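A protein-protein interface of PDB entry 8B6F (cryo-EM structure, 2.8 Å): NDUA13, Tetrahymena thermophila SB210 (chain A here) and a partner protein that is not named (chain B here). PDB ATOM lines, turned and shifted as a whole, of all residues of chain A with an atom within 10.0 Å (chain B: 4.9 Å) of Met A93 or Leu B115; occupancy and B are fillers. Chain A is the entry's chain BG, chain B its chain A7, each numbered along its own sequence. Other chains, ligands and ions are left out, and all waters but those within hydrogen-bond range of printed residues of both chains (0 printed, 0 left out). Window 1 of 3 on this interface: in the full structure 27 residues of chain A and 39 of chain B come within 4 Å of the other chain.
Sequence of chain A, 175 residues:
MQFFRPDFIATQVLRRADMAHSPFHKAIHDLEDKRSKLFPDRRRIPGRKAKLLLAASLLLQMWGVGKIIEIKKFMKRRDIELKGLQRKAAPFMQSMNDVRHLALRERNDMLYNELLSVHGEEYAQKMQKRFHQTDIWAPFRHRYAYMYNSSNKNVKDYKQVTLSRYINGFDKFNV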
ATOM      1  N   LEU A  82      31.804  20.499  -5.298  1.00  0.00           N
ATOM      2  CA  LEU A  82      30.622  20.040  -4.577  1.00  0.00           C
ATOM      3  C   LEU A  82      30.812  20.205  -3.076  1.00  0.00           C
ATOM      4  O   LEU A  82      29.896  20.634  -2.367  1.00  0.00           O
ATOM      5  CB  LEU A  82      30.312  18.582  -4.916  1.00  0.00           C
ATOM      6  CG  LEU A  82      29.036  18.040  -4.254  1.00  0.00           C
ATOM      7  CD1 LEU A  82      27.778  18.663  -4.829  1.00  0.00           C
ATOM      8  CD2 LEU A  82      28.975  16.538  -4.375  1.00  0.00           C
ATOM      9  N   GLY A  84      32.723  22.420  -1.668  1.00  0.00           N
ATOM     10  CA  GLY A  84      32.622  23.845  -1.399  1.00  0.00           C
ATOM     11  C   GLY A  84      31.184  24.308  -1.264  1.00  0.00           C
ATOM     12  O   GLY A  84      30.845  25.066  -0.353  1.00  0.00           O
ATOM     13  N   LEU A  85      30.317  23.861  -2.174  1.00  0.00           N
ATOM     14  CA  LEU A  85      28.905  24.220  -2.085  1.00  0.00           C
ATOM     15  C   LEU A  85      28.282  23.671  -0.810  1.00  0.00           C
ATOM     16  O   LEU A  85      27.506  24.360  -0.140  1.00  0.00           O
ATOM     17  CB  LEU A  85      28.153  23.708  -3.312  1.00  0.00           C
ATOM     18  CG  LEU A  85      28.599  24.277  -4.659  1.00  0.00           C
ATOM     19  CD1 LEU A  85      27.828  23.620  -5.786  1.00  0.00           C
ATOM     20  CD2 LEU A  85      28.426  25.786  -4.703  1.00  0.00           C
ATOM     21  N   GLN A  86      28.609  22.426  -0.460  1.00  0.00           N
ATOM     22  CA  GLN A  86      28.087  21.836   0.767  1.00  0.00           C
ATOM     23  C   GLN A  86      28.557  22.610   1.991  1.00  0.00           C
ATOM     24  O   GLN A  86      27.799  22.793   2.950  1.00  0.00           O
ATOM     25  CB  GLN A  86      28.503  20.367   0.859  1.00  0.00           C
ATOM     26  CG  GLN A  86      27.851  19.485  -0.193  1.00  0.00           C
ATOM     27  CD  GLN A  86      28.387  18.071  -0.180  1.00  0.00           C
ATOM     28  OE1 GLN A  86      29.466  17.809   0.348  1.00  0.00           O
ATOM     29  NE2 GLN A  86      27.629  17.148  -0.757  1.00  0.00           N
ATOM     30  N   ARG A  87      29.807  23.074   1.975  1.00  0.00           N
ATOM     31  CA  ARG A  87      30.304  23.909   3.063  1.00  0.00           C
ATOM     32  C   ARG A  87      29.521  25.212   3.158  1.00  0.00           C
ATOM     33  O   ARG A  87      29.180  25.658   4.258  1.00  0.00           O
ATOM     34  CB  ARG A  87      31.794  24.193   2.864  1.00  0.00           C
ATOM     35  CG  ARG A  87      32.402  25.128   3.902  1.00  0.00           C
ATOM     36  CD  ARG A  87      32.413  26.578   3.431  1.00  0.00           C
ATOM     37  NE  ARG A  87      33.032  27.460   4.412  1.00  0.00           N
ATOM     38  CZ  ARG A  87      32.409  27.970   5.467  1.00  0.00           C
ATOM     39  NH1 ARG A  87      31.140  27.698   5.718  1.00  0.00           N
ATOM     40  NH2 ARG A  87      33.077  28.774   6.289  1.00  0.00           N
ATOM     41  N   LYS A  88      29.231  25.840   2.017  1.00  0.00           N
ATOM     42  CA  LYS A  88      28.433  27.062   2.035  1.00  0.00           C
ATOM     43  C   LYS A  88      27.073  26.821   2.678  1.00  0.00           C
ATOM     44  O   LYS A  88      26.584  27.655   3.447  1.00  0.00           O
ATOM     45  CB  LYS A  88      28.260  27.590   0.611  1.00  0.00           C
ATOM     46  CG  LYS A  88      29.434  28.404   0.091  1.00  0.00           C
ATOM     47  CD  LYS A  88      29.079  29.093  -1.218  1.00  0.00           C
ATOM     48  CE  LYS A  88      30.205  29.991  -1.697  1.00  0.00           C
ATOM     49  NZ  LYS A  88      29.858  30.679  -2.972  1.00  0.00           N
ATOM     50  N   ALA A  89      26.442  25.690   2.369  1.00  0.00           N
ATOM     51  CA  ALA A  89      25.118  25.386   2.896  1.00  0.00           C
ATOM     52  C   ALA A  89      25.146  24.834   4.315  1.00  0.00           C
ATOM     53  O   ALA A  89      24.095  24.789   4.964  1.00  0.00           O
ATOM     54  CB  ALA A  89      24.415  24.384   1.977  1.00  0.00           C
ATOM     55  N   ALA A  90      26.310  24.418   4.812  1.00  0.00           N
ATOM     56  CA  ALA A  90      26.362  23.699   6.083  1.00  0.00           C
ATOM     57  C   ALA A  90      25.887  24.529   7.267  1.00  0.00           C
ATOM     58  O   ALA A  90      25.044  24.036   8.035  1.00  0.00           O
ATOM     59  CB  ALA A  90      27.784  23.183   6.319  1.00  0.00           C
ATOM     60  N   PRO A  91      26.371  25.756   7.489  1.00  0.00           N
ATOM     61  CA  PRO A  91      26.110  26.405   8.787  1.00  0.00           C
ATOM     62  C   PRO A  91      24.635  26.557   9.120  1.00  0.00           C
ATOM     63  O   PRO A  91      24.257  26.427  10.289  1.00  0.00           O
ATOM     64  CB  PRO A  91      26.810  27.768   8.648  1.00  0.00           C
ATOM     65  CG  PRO A  91      26.993  27.973   7.193  1.00  0.00           C
ATOM     66  CD  PRO A  91      27.171  26.616   6.599  1.00  0.00           C
ATOM     67  N   PHE A  92      23.788  26.833   8.129  1.00  0.00           N
ATOM     68  CA  PHE A  92      22.381  27.092   8.419  1.00  0.00           C
ATOM     69  C   PHE A  92      21.662  25.820   8.846  1.00  0.00           C
ATOM     70  O   PHE A  92      20.905  25.822   9.824  1.00  0.00           O
ATOM     71  CB  PHE A  92      21.707  27.712   7.200  1.00  0.00           C
ATOM     72  CG  PHE A  92      22.391  28.947   6.707  1.00  0.00           C
ATOM     73  CD1 PHE A  92      22.110  30.171   7.277  1.00  0.00           C
ATOM     74  CD2 PHE A  92      23.326  28.882   5.691  1.00  0.00           C
ATOM     75  CE1 PHE A  92      22.736  31.310   6.838  1.00  0.00           C
ATOM     76  CE2 PHE A  92      23.958  30.023   5.246  1.00  0.00           C
ATOM     77  CZ  PHE A  92      23.664  31.239   5.823  1.00  0.00           C
ATOM     78  N   MET A  93      21.884  24.721   8.128  1.00  0.00           N
ATOM     79  CA  MET A  93      21.272  23.457   8.518  1.00  0.00           C
ATOM     80  C   MET A  93      21.775  23.008   9.882  1.00  0.00           C
ATOM     81  O   MET A  93      21.012  22.465  10.688  1.00  0.00           O
ATOM     82  CB  MET A  93      21.543  22.391   7.460  1.00  0.00           C
ATOM     83  CG  MET A  93      21.091  22.800   6.073  1.00  0.00           C
ATOM     84  SD  MET A  93      21.179  21.450   4.891  1.00  0.00           S
ATOM     85  CE  MET A  93      19.833  20.414   5.449  1.00  0.00           C
ATOM     86  N   GLN A  94      23.064  23.213  10.151  1.00  0.00           N
ATOM     87  CA  GLN A  94      23.604  22.889  11.464  1.00  0.00           C
ATOM     88  C   GLN A  94      22.922  23.707  12.552  1.00  0.00           C
ATOM     89  O   GLN A  94      22.599  23.184  13.624  1.00  0.00           O
ATOM     90  CB  GLN A  94      25.114  23.125  11.478  1.00  0.00           C
ATOM     91  CG  GLN A  94      25.814  22.631  12.732  1.00  0.00           C
ATOM     92  CD  GLN A  94      25.784  21.121  12.856  1.00  0.00           C
ATOM     93  OE1 GLN A  94      25.338  20.423  11.950  1.00  0.00           O
ATOM     94  NE2 GLN A  94      26.263  20.611  13.982  1.00  0.00           N
ATOM     95  N   SER A  95      22.695  24.998  12.298  1.00  0.00           N
ATOM     96  CA  SER A  95      22.031  25.836  13.290  1.00  0.00           C
ATOM     97  C   SER A  95      20.613  25.349  13.556  1.00  0.00           C
ATOM     98  O   SER A  95      20.182  25.260  14.711  1.00  0.00           O
ATOM     99  CB  SER A  95      22.016  27.289  12.817  1.00  0.00           C
ATOM    100  OG  SER A  95      23.331  27.768  12.596  1.00  0.00           O
ATOM    101  N   MET A  96      19.867  25.031  12.496  1.00  0.00           N
ATOM    102  CA  MET A  96      18.507  24.539  12.682  1.00  0.00           C
ATOM    103  C   MET A  96      18.506  23.236  13.467  1.00  0.00           C
ATOM    104  O   MET A  96      17.704  23.056  14.389  1.00  0.00           O
ATOM    105  CB  MET A  96      17.826  24.344  11.329  1.00  0.00           C
ATOM    106  CG  MET A  96      17.766  25.597  10.481  1.00  0.00           C
ATOM    107  SD  MET A  96      17.152  25.279   8.820  1.00  0.00           S
ATOM    108  CE  MET A  96      17.808  26.702   7.956  1.00  0.00           C
ATOM    109  N   ASN A  97      19.403  22.317  13.113  1.00  0.00           N
ATOM    110  CA  ASN A  97      19.476  21.041  13.814  1.00  0.00           C
ATOM    111  C   ASN A  97      19.827  21.240  15.281  1.00  0.00           C
ATOM    112  O   ASN A  97      19.249  20.589  16.160  1.00  0.00           O
ATOM    113  CB  ASN A  97      20.504  20.137  13.134  1.00  0.00           C
ATOM    114  CG  ASN A  97      20.618  18.785  13.799  1.00  0.00           C
ATOM    115  OD1 ASN A  97      19.894  17.850  13.459  1.00  0.00           O
ATOM    116  ND2 ASN A  97      21.533  18.671  14.750  1.00  0.00           N
ATOM    117  N   ASP A  98      20.777  22.132  15.566  1.00  0.00           N
ATOM    118  CA  ASP A  98      21.149  22.397  16.951  1.00  0.00           C
ATOM    119  C   ASP A  98      19.987  22.986  17.740  1.00  0.00           C
ATOM    120  O   ASP A  98      19.761  22.608  18.895  1.00  0.00           O
ATOM    121  CB  ASP A  98      22.352  23.339  16.996  1.00  0.00           C
ATOM    122  CG  ASP A  98      23.629  22.674  16.527  1.00  0.00           C
ATOM    123  OD1 ASP A  98      23.568  21.505  16.096  1.00  0.00           O
ATOM    124  OD2 ASP A  98      24.696  23.318  16.598  1.00  0.00           O
ATOM    125  N   VAL A  99      19.234  23.906  17.136  1.00  0.00           N
ATOM    126  CA  VAL A  99      18.107  24.507  17.843  1.00  0.00           C
ATOM    127  C   VAL A  99      17.059  23.452  18.171  1.00  0.00           C
ATOM    128  O   VAL A  99      16.529  23.411  19.288  1.00  0.00           O
ATOM    129  CB  VAL A  99      17.514  25.665  17.020  1.00  0.00           C
ATOM    130  CG1 VAL A  99      16.166  26.083  17.575  1.00  0.00           C
ATOM    131  CG2 VAL A  99      18.469  26.841  17.007  1.00  0.00           C
ATOM    132  N   ARG A 100      16.735  22.589  17.207  1.00  0.00           N
ATOM    133  CA  ARG A 100      15.763  21.536  17.470  1.00  0.00           C
ATOM    134  C   ARG A 100      16.269  20.589  18.549  1.00  0.00           C
ATOM    135  O   ARG A 100      15.518  20.191  19.444  1.00  0.00           O
ATOM    136  CB  ARG A 100      15.455  20.769  16.186  1.00  0.00           C
ATOM    137  CG  ARG A 100      14.767  21.599  15.117  1.00  0.00           C
ATOM    138  CD  ARG A 100      14.324  20.719  13.964  1.00  0.00           C
ATOM    139  NE  ARG A 100      13.592  21.457  12.942  1.00  0.00           N
ATOM    140  CZ  ARG A 100      14.136  21.983  11.853  1.00  0.00           C
ATOM    141  NH1 ARG A 100      15.432  21.888  11.610  1.00  0.00           N
ATOM    142  NH2 ARG A 100      13.357  22.611  10.978  1.00  0.00           N
ATOM    143  N   HIS A 101      17.548  20.219  18.475  1.00  0.00           N
ATOM    144  CA  HIS A 101      18.127  19.324  19.469  1.00  0.00           C
ATOM    145  C   HIS A 101      18.055  19.932  20.862  1.00  0.00           C
ATOM    146  O   HIS A 101      17.721  19.246  21.833  1.00  0.00           O
ATOM    147  CB  HIS A 101      19.573  19.010  19.088  1.00  0.00           C
ATOM    148  CG  HIS A 101      20.231  17.998  19.972  1.00  0.00           C
ATOM    149  ND1 HIS A 101      21.099  18.346  20.982  1.00  0.00           N
ATOM    150  CD2 HIS A 101      20.152  16.647  19.992  1.00  0.00           C
ATOM    151  CE1 HIS A 101      21.526  17.255  21.589  1.00  0.00           C
ATOM    152  NE2 HIS A 101      20.969  16.209  21.007  1.00  0.00           N
ATOM    153  N   ASN A 174      10.646  16.732  -1.070  1.00  0.00           N
ATOM    154  CA  ASN A 174      11.369  17.688  -0.234  1.00  0.00           C
ATOM    155  C   ASN A 174      11.713  18.981  -0.970  1.00  0.00           C
ATOM    156  O   ASN A 174      12.337  19.874  -0.390  1.00  0.00           O
ATOM    157  CB  ASN A 174      12.660  17.059   0.298  1.00  0.00           C
ATOM    158  CG  ASN A 174      12.401  15.907   1.247  1.00  0.00           C
ATOM    159  OD1 ASN A 174      11.343  15.827   1.871  1.00  0.00           O
ATOM    160  ND2 ASN A 174      13.374  15.012   1.367  1.00  0.00           N
ATOM    161  N   VAL A 175      11.357  19.084  -2.245  1.00  0.00           N
ATOM    162  CA  VAL A 175      11.343  20.375  -2.921  1.00  0.00           C
ATOM    163  C   VAL A 175       9.931  20.942  -2.848  1.00  0.00           C
ATOM    164  O   VAL A 175       8.961  20.275  -3.203  1.00  0.00           O
ATOM    165  CB  VAL A 175      11.823  20.258  -4.377  1.00  0.00           C
ATOM    166  CG1 VAL A 175      11.194  21.327  -5.263  1.00  0.00           C
ATOM    167  CG2 VAL A 175      13.323  20.366  -4.433  1.00  0.00           C
ATOM    168  OXT VAL A 175       9.725  22.085  -2.441  1.00  0.00           O
ATOM    169  N   SER B 111      14.266  20.858   2.829  1.00  0.00           N
ATOM    170  CA  SER B 111      15.723  20.787   2.879  1.00  0.00           C
ATOM    171  C   SER B 111      16.364  21.401   1.641  1.00  0.00           C
ATOM    172  O   SER B 111      17.264  22.240   1.747  1.00  0.00           O
ATOM    173  CB  SER B 111      16.161  19.332   3.037  1.00  0.00           C
ATOM    174  OG  SER B 111      17.571  19.240   3.128  1.00  0.00           O
ATOM    175  N   PHE B 112      15.919  20.991   0.451  1.00  0.00           N
ATOM    176  CA  PHE B 112      16.567  21.457  -0.771  1.00  0.00           C
ATOM    177  C   PHE B 112      16.386  22.959  -0.953  1.00  0.00           C
ATOM    178  O   PHE B 112      17.314  23.651  -1.385  1.00  0.00           O
ATOM    179  CB  PHE B 112      16.039  20.686  -1.982  1.00  0.00           C
ATOM    180  CG  PHE B 112      16.361  19.208  -1.956  1.00  0.00           C
ATOM    181  CD1 PHE B 112      17.219  18.678  -1.005  1.00  0.00           C
ATOM    182  CD2 PHE B 112      15.816  18.354  -2.901  1.00  0.00           C
ATOM    183  CE1 PHE B 112      17.512  17.328  -0.992  1.00  0.00           C
ATOM    184  CE2 PHE B 112      16.104  17.007  -2.891  1.00  0.00           C
ATOM    185  CZ  PHE B 112      16.952  16.493  -1.937  1.00  0.00           C
ATOM    186  N   GLU B 113      15.205  23.483  -0.626  1.00  0.00           N
ATOM    187  CA  GLU B 113      15.007  24.929  -0.666  1.00  0.00           C
ATOM    188  C   GLU B 113      15.923  25.632   0.327  1.00  0.00           C
ATOM    189  O   GLU B 113      16.433  26.723   0.049  1.00  0.00           O
ATOM    190  CB  GLU B 113      13.546  25.268  -0.383  1.00  0.00           C
ATOM    191  CG  GLU B 113      12.581  24.688  -1.400  1.00  0.00           C
ATOM    192  CD  GLU B 113      11.144  25.044  -1.097  1.00  0.00           C
ATOM    193  OE1 GLU B 113      10.909  25.756  -0.101  1.00  0.00           O
ATOM    194  OE2 GLU B 113      10.250  24.611  -1.853  1.00  0.00           O
ATOM    195  N   VAL B 114      16.145  25.023   1.493  1.00  0.00           N
ATOM    196  CA  VAL B 114      17.070  25.597   2.466  1.00  0.00           C
ATOM    197  C   VAL B 114      18.475  25.656   1.884  1.00  0.00           C
ATOM    198  O   VAL B 114      19.192  26.648   2.054  1.00  0.00           O
ATOM    199  CB  VAL B 114      17.028  24.800   3.783  1.00  0.00           C
ATOM    200  CG1 VAL B 114      18.214  25.150   4.675  1.00  0.00           C
ATOM    201  CG2 VAL B 114      15.732  25.076   4.523  1.00  0.00           C
ATOM    202  N   LEU B 115      18.897  24.593   1.198  1.00  0.00           N
ATOM    203  CA  LEU B 115      20.212  24.599   0.565  1.00  0.00           C
ATOM    204  C   LEU B 115      20.308  25.704  -0.479  1.00  0.00           C
ATOM    205  O   LEU B 115      21.303  26.435  -0.538  1.00  0.00           O
ATOM    206  CB  LEU B 115      20.494  23.241  -0.077  1.00  0.00           C
ATOM    207  CG  LEU B 115      20.592  22.033   0.854  1.00  0.00           C
ATOM    208  CD1 LEU B 115      20.612  20.744   0.056  1.00  0.00           C
ATOM    209  CD2 LEU B 115      21.821  22.134   1.729  1.00  0.00           C
ATOM    210  N   ILE B 116      19.279  25.841  -1.316  1.00  0.00           N
ATOM    211  CA  ILE B 116      19.303  26.858  -2.365  1.00  0.00           C
ATOM    212  C   ILE B 116      19.411  28.247  -1.749  1.00  0.00           C
ATOM    213  O   ILE B 116      20.204  29.084  -2.195  1.00  0.00           O
ATOM    214  CB  ILE B 116      18.057  26.730  -3.259  1.00  0.00           C
ATOM    215  CG1 ILE B 116      18.071  25.390  -3.996  1.00  0.00           C
ATOM    216  CG2 ILE B 116      17.988  27.878  -4.259  1.00  0.00           C
ATOM    217  CD1 ILE B 116      16.757  25.039  -4.651  1.00  0.00           C
ATOM    218  N   HIS B 117      18.618  28.508  -0.710  1.00  0.00           N
ATOM    219  CA  HIS B 117      18.669  29.807  -0.048  1.00  0.00           C
ATOM    220  C   HIS B 117      20.017  30.034   0.620  1.00  0.00           C
ATOM    221  O   HIS B 117      20.561  31.143   0.578  1.00  0.00           O
ATOM    222  CB  HIS B 117      17.540  29.920   0.975  1.00  0.00           C
ATOM    223  CG  HIS B 117      16.218  30.281   0.376  1.00  0.00           C
ATOM    224  ND1 HIS B 117      15.052  29.616   0.688  1.00  0.00           N
ATOM    225  CD2 HIS B 117      15.874  31.247  -0.508  1.00  0.00           C
ATOM    226  CE1 HIS B 117      14.049  30.151   0.017  1.00  0.00           C
ATOM    227  NE2 HIS B 117      14.520  31.144  -0.717  1.00  0.00           N
ATOM    228  N   SER B 118      20.578  28.992   1.235  1.00  0.00           N
ATOM    229  CA  SER B 118      21.868  29.141   1.897  1.00  0.00           C
ATOM    230  C   SER B 118      22.970  29.486   0.908  1.00  0.00           C
ATOM    231  O   SER B 118      23.892  30.236   1.246  1.00  0.00           O
ATOM    232  CB  SER B 118      22.223  27.855   2.644  1.00  0.00           C
ATOM    233  OG  SER B 118      21.256  27.554   3.633  1.00  0.00           O
ATOM    234  N   GLN B 119      22.898  28.952  -0.313  1.00  0.00           N
ATOM    235  CA  GLN B 119      23.939  29.232  -1.295  1.00  0.00           C
ATOM    236  C   GLN B 119      24.091  30.727  -1.542  1.00  0.00           C
ATOM    237  O   GLN B 119      25.169  31.182  -1.938  1.00  0.00           O
ATOM    238  CB  GLN B 119      23.632  28.500  -2.603  1.00  0.00           C
ATOM    239  CG  GLN B 119      23.828  26.993  -2.521  1.00  0.00           C
ATOM    240  CD  GLN B 119      25.249  26.603  -2.183  1.00  0.00           C
ATOM    241  OE1 GLN B 119      26.178  27.388  -2.366  1.00  0.00           O
ATOM    242  NE2 GLN B 119      25.425  25.389  -1.678  1.00  0.00           N
ATOM    243  N   MET B 181      16.711  20.574  -8.411  1.00  0.00           N
ATOM    244  CA  MET B 181      17.048  19.899  -7.164  1.00  0.00           C
ATOM    245  C   MET B 181      16.025  18.838  -6.783  1.00  0.00           C
ATOM    246  O   MET B 181      16.316  17.996  -5.929  1.00  0.00           O
ATOM    247  CB  MET B 181      17.177  20.917  -6.031  1.00  0.00           C
ATOM    248  CG  MET B 181      18.405  21.803  -6.139  1.00  0.00           C
ATOM    249  SD  MET B 181      19.944  20.901  -5.870  1.00  0.00           S
ATOM    250  CE  MET B 181      19.823  20.525  -4.124  1.00  0.00           C
ATOM    251  N   LEU B 188      23.940  19.173  -5.523  1.00  0.00           N
ATOM    252  CA  LEU B 188      24.109  20.610  -5.709  1.00  0.00           C
ATOM    253  C   LEU B 188      24.943  20.920  -6.945  1.00  0.00           C
ATOM    254  O   LEU B 188      24.685  21.908  -7.640  1.00  0.00           O
ATOM    255  CB  LEU B 188      24.750  21.226  -4.466  1.00  0.00           C
ATOM    256  CG  LEU B 188      23.859  21.357  -3.228  1.00  0.00           C
ATOM    257  CD1 LEU B 188      24.688  21.712  -2.008  1.00  0.00           C
ATOM    258  CD2 LEU B 188      22.777  22.400  -3.451  1.00  0.00           C
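Among the printed residues, merely in contact across the chains: Leu A82 with Leu B188, Lys A88 with Gln B119, Ala A89 with Leu B115, Ala A89 with Ser B118, Ala A89 with Gln B119, Phe A92 with Ser B118, Met A93 with Ser B111, Met A93 with Val B114, Met A93 with Leu B115, Met A96 with Val B114, Asn A174 with Ser B111, Asn A174 with Phe B112, Val A175 with Phe B112 and Val A175 with Met B181.
OXT of Val A175 lies close to OE2 of Glu B113.
NE2 of Gln B119 lies within hydrogen-bond range of O of Leu A85, at 2.8 Å.
Hydrophobic or aromatic side chains of chain B within 4 Å of the printed part of chain A: Phe B112, Val B114, Leu B115 and Leu B188.
Of the 21 printed residues of chain A, 9 touch a printed residue of chain B.
Hydrophobic or aromatic side chains of chain A that line the printed part of chain B: Leu A82, Leu A85, Ala A89, Phe A92, Met A93, Met A96 and Val A175.
Among the printed residues, 16 pairs touch across the chains.
Printed residues of chain B within 4 Å of Leu A82: Leu B188 (3.9 Å).
Ala A90 touches none of the printed residues of chain B.
Of the printed residues of chain B, Phe A92 touches Ser B118.
Of chain B, only Ser B111, Val B114 and Leu B115 come within 4 Å of Met A93.
Of the printed residues of chain A, Val B114 touches Met A93 (3.97 Å) and Met A96 (3.7 Å).
Of chain A, only Ala A89 (3.4 Å) and Met A93 (3.3 Å) come within 4 Å of Leu B115.
No residue of chain A comes within 4 Å of Ile B116.
Of chain A, only Ala A89 (3.8 Å) and Phe A92 (3.2 Å) come within 4 Å of Ser B118.
Of the printed residues of chain A, Met B181 touches Val A175 (3.9 Å).
The nearest printed residue of chain B that does not touch Met A93 is Ser B118 (5.3 Å).
The nearest printed residue of chain B that does not touch Asn A174 is Glu B113 (4.6 Å).
OG of Ser B118 lies within hydrogen-bond range of O of Val B114 (2.8 Å).
O of Glu B113 lies within hydrogen-bond range of ND1 of His B117, at 3.3 Å.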
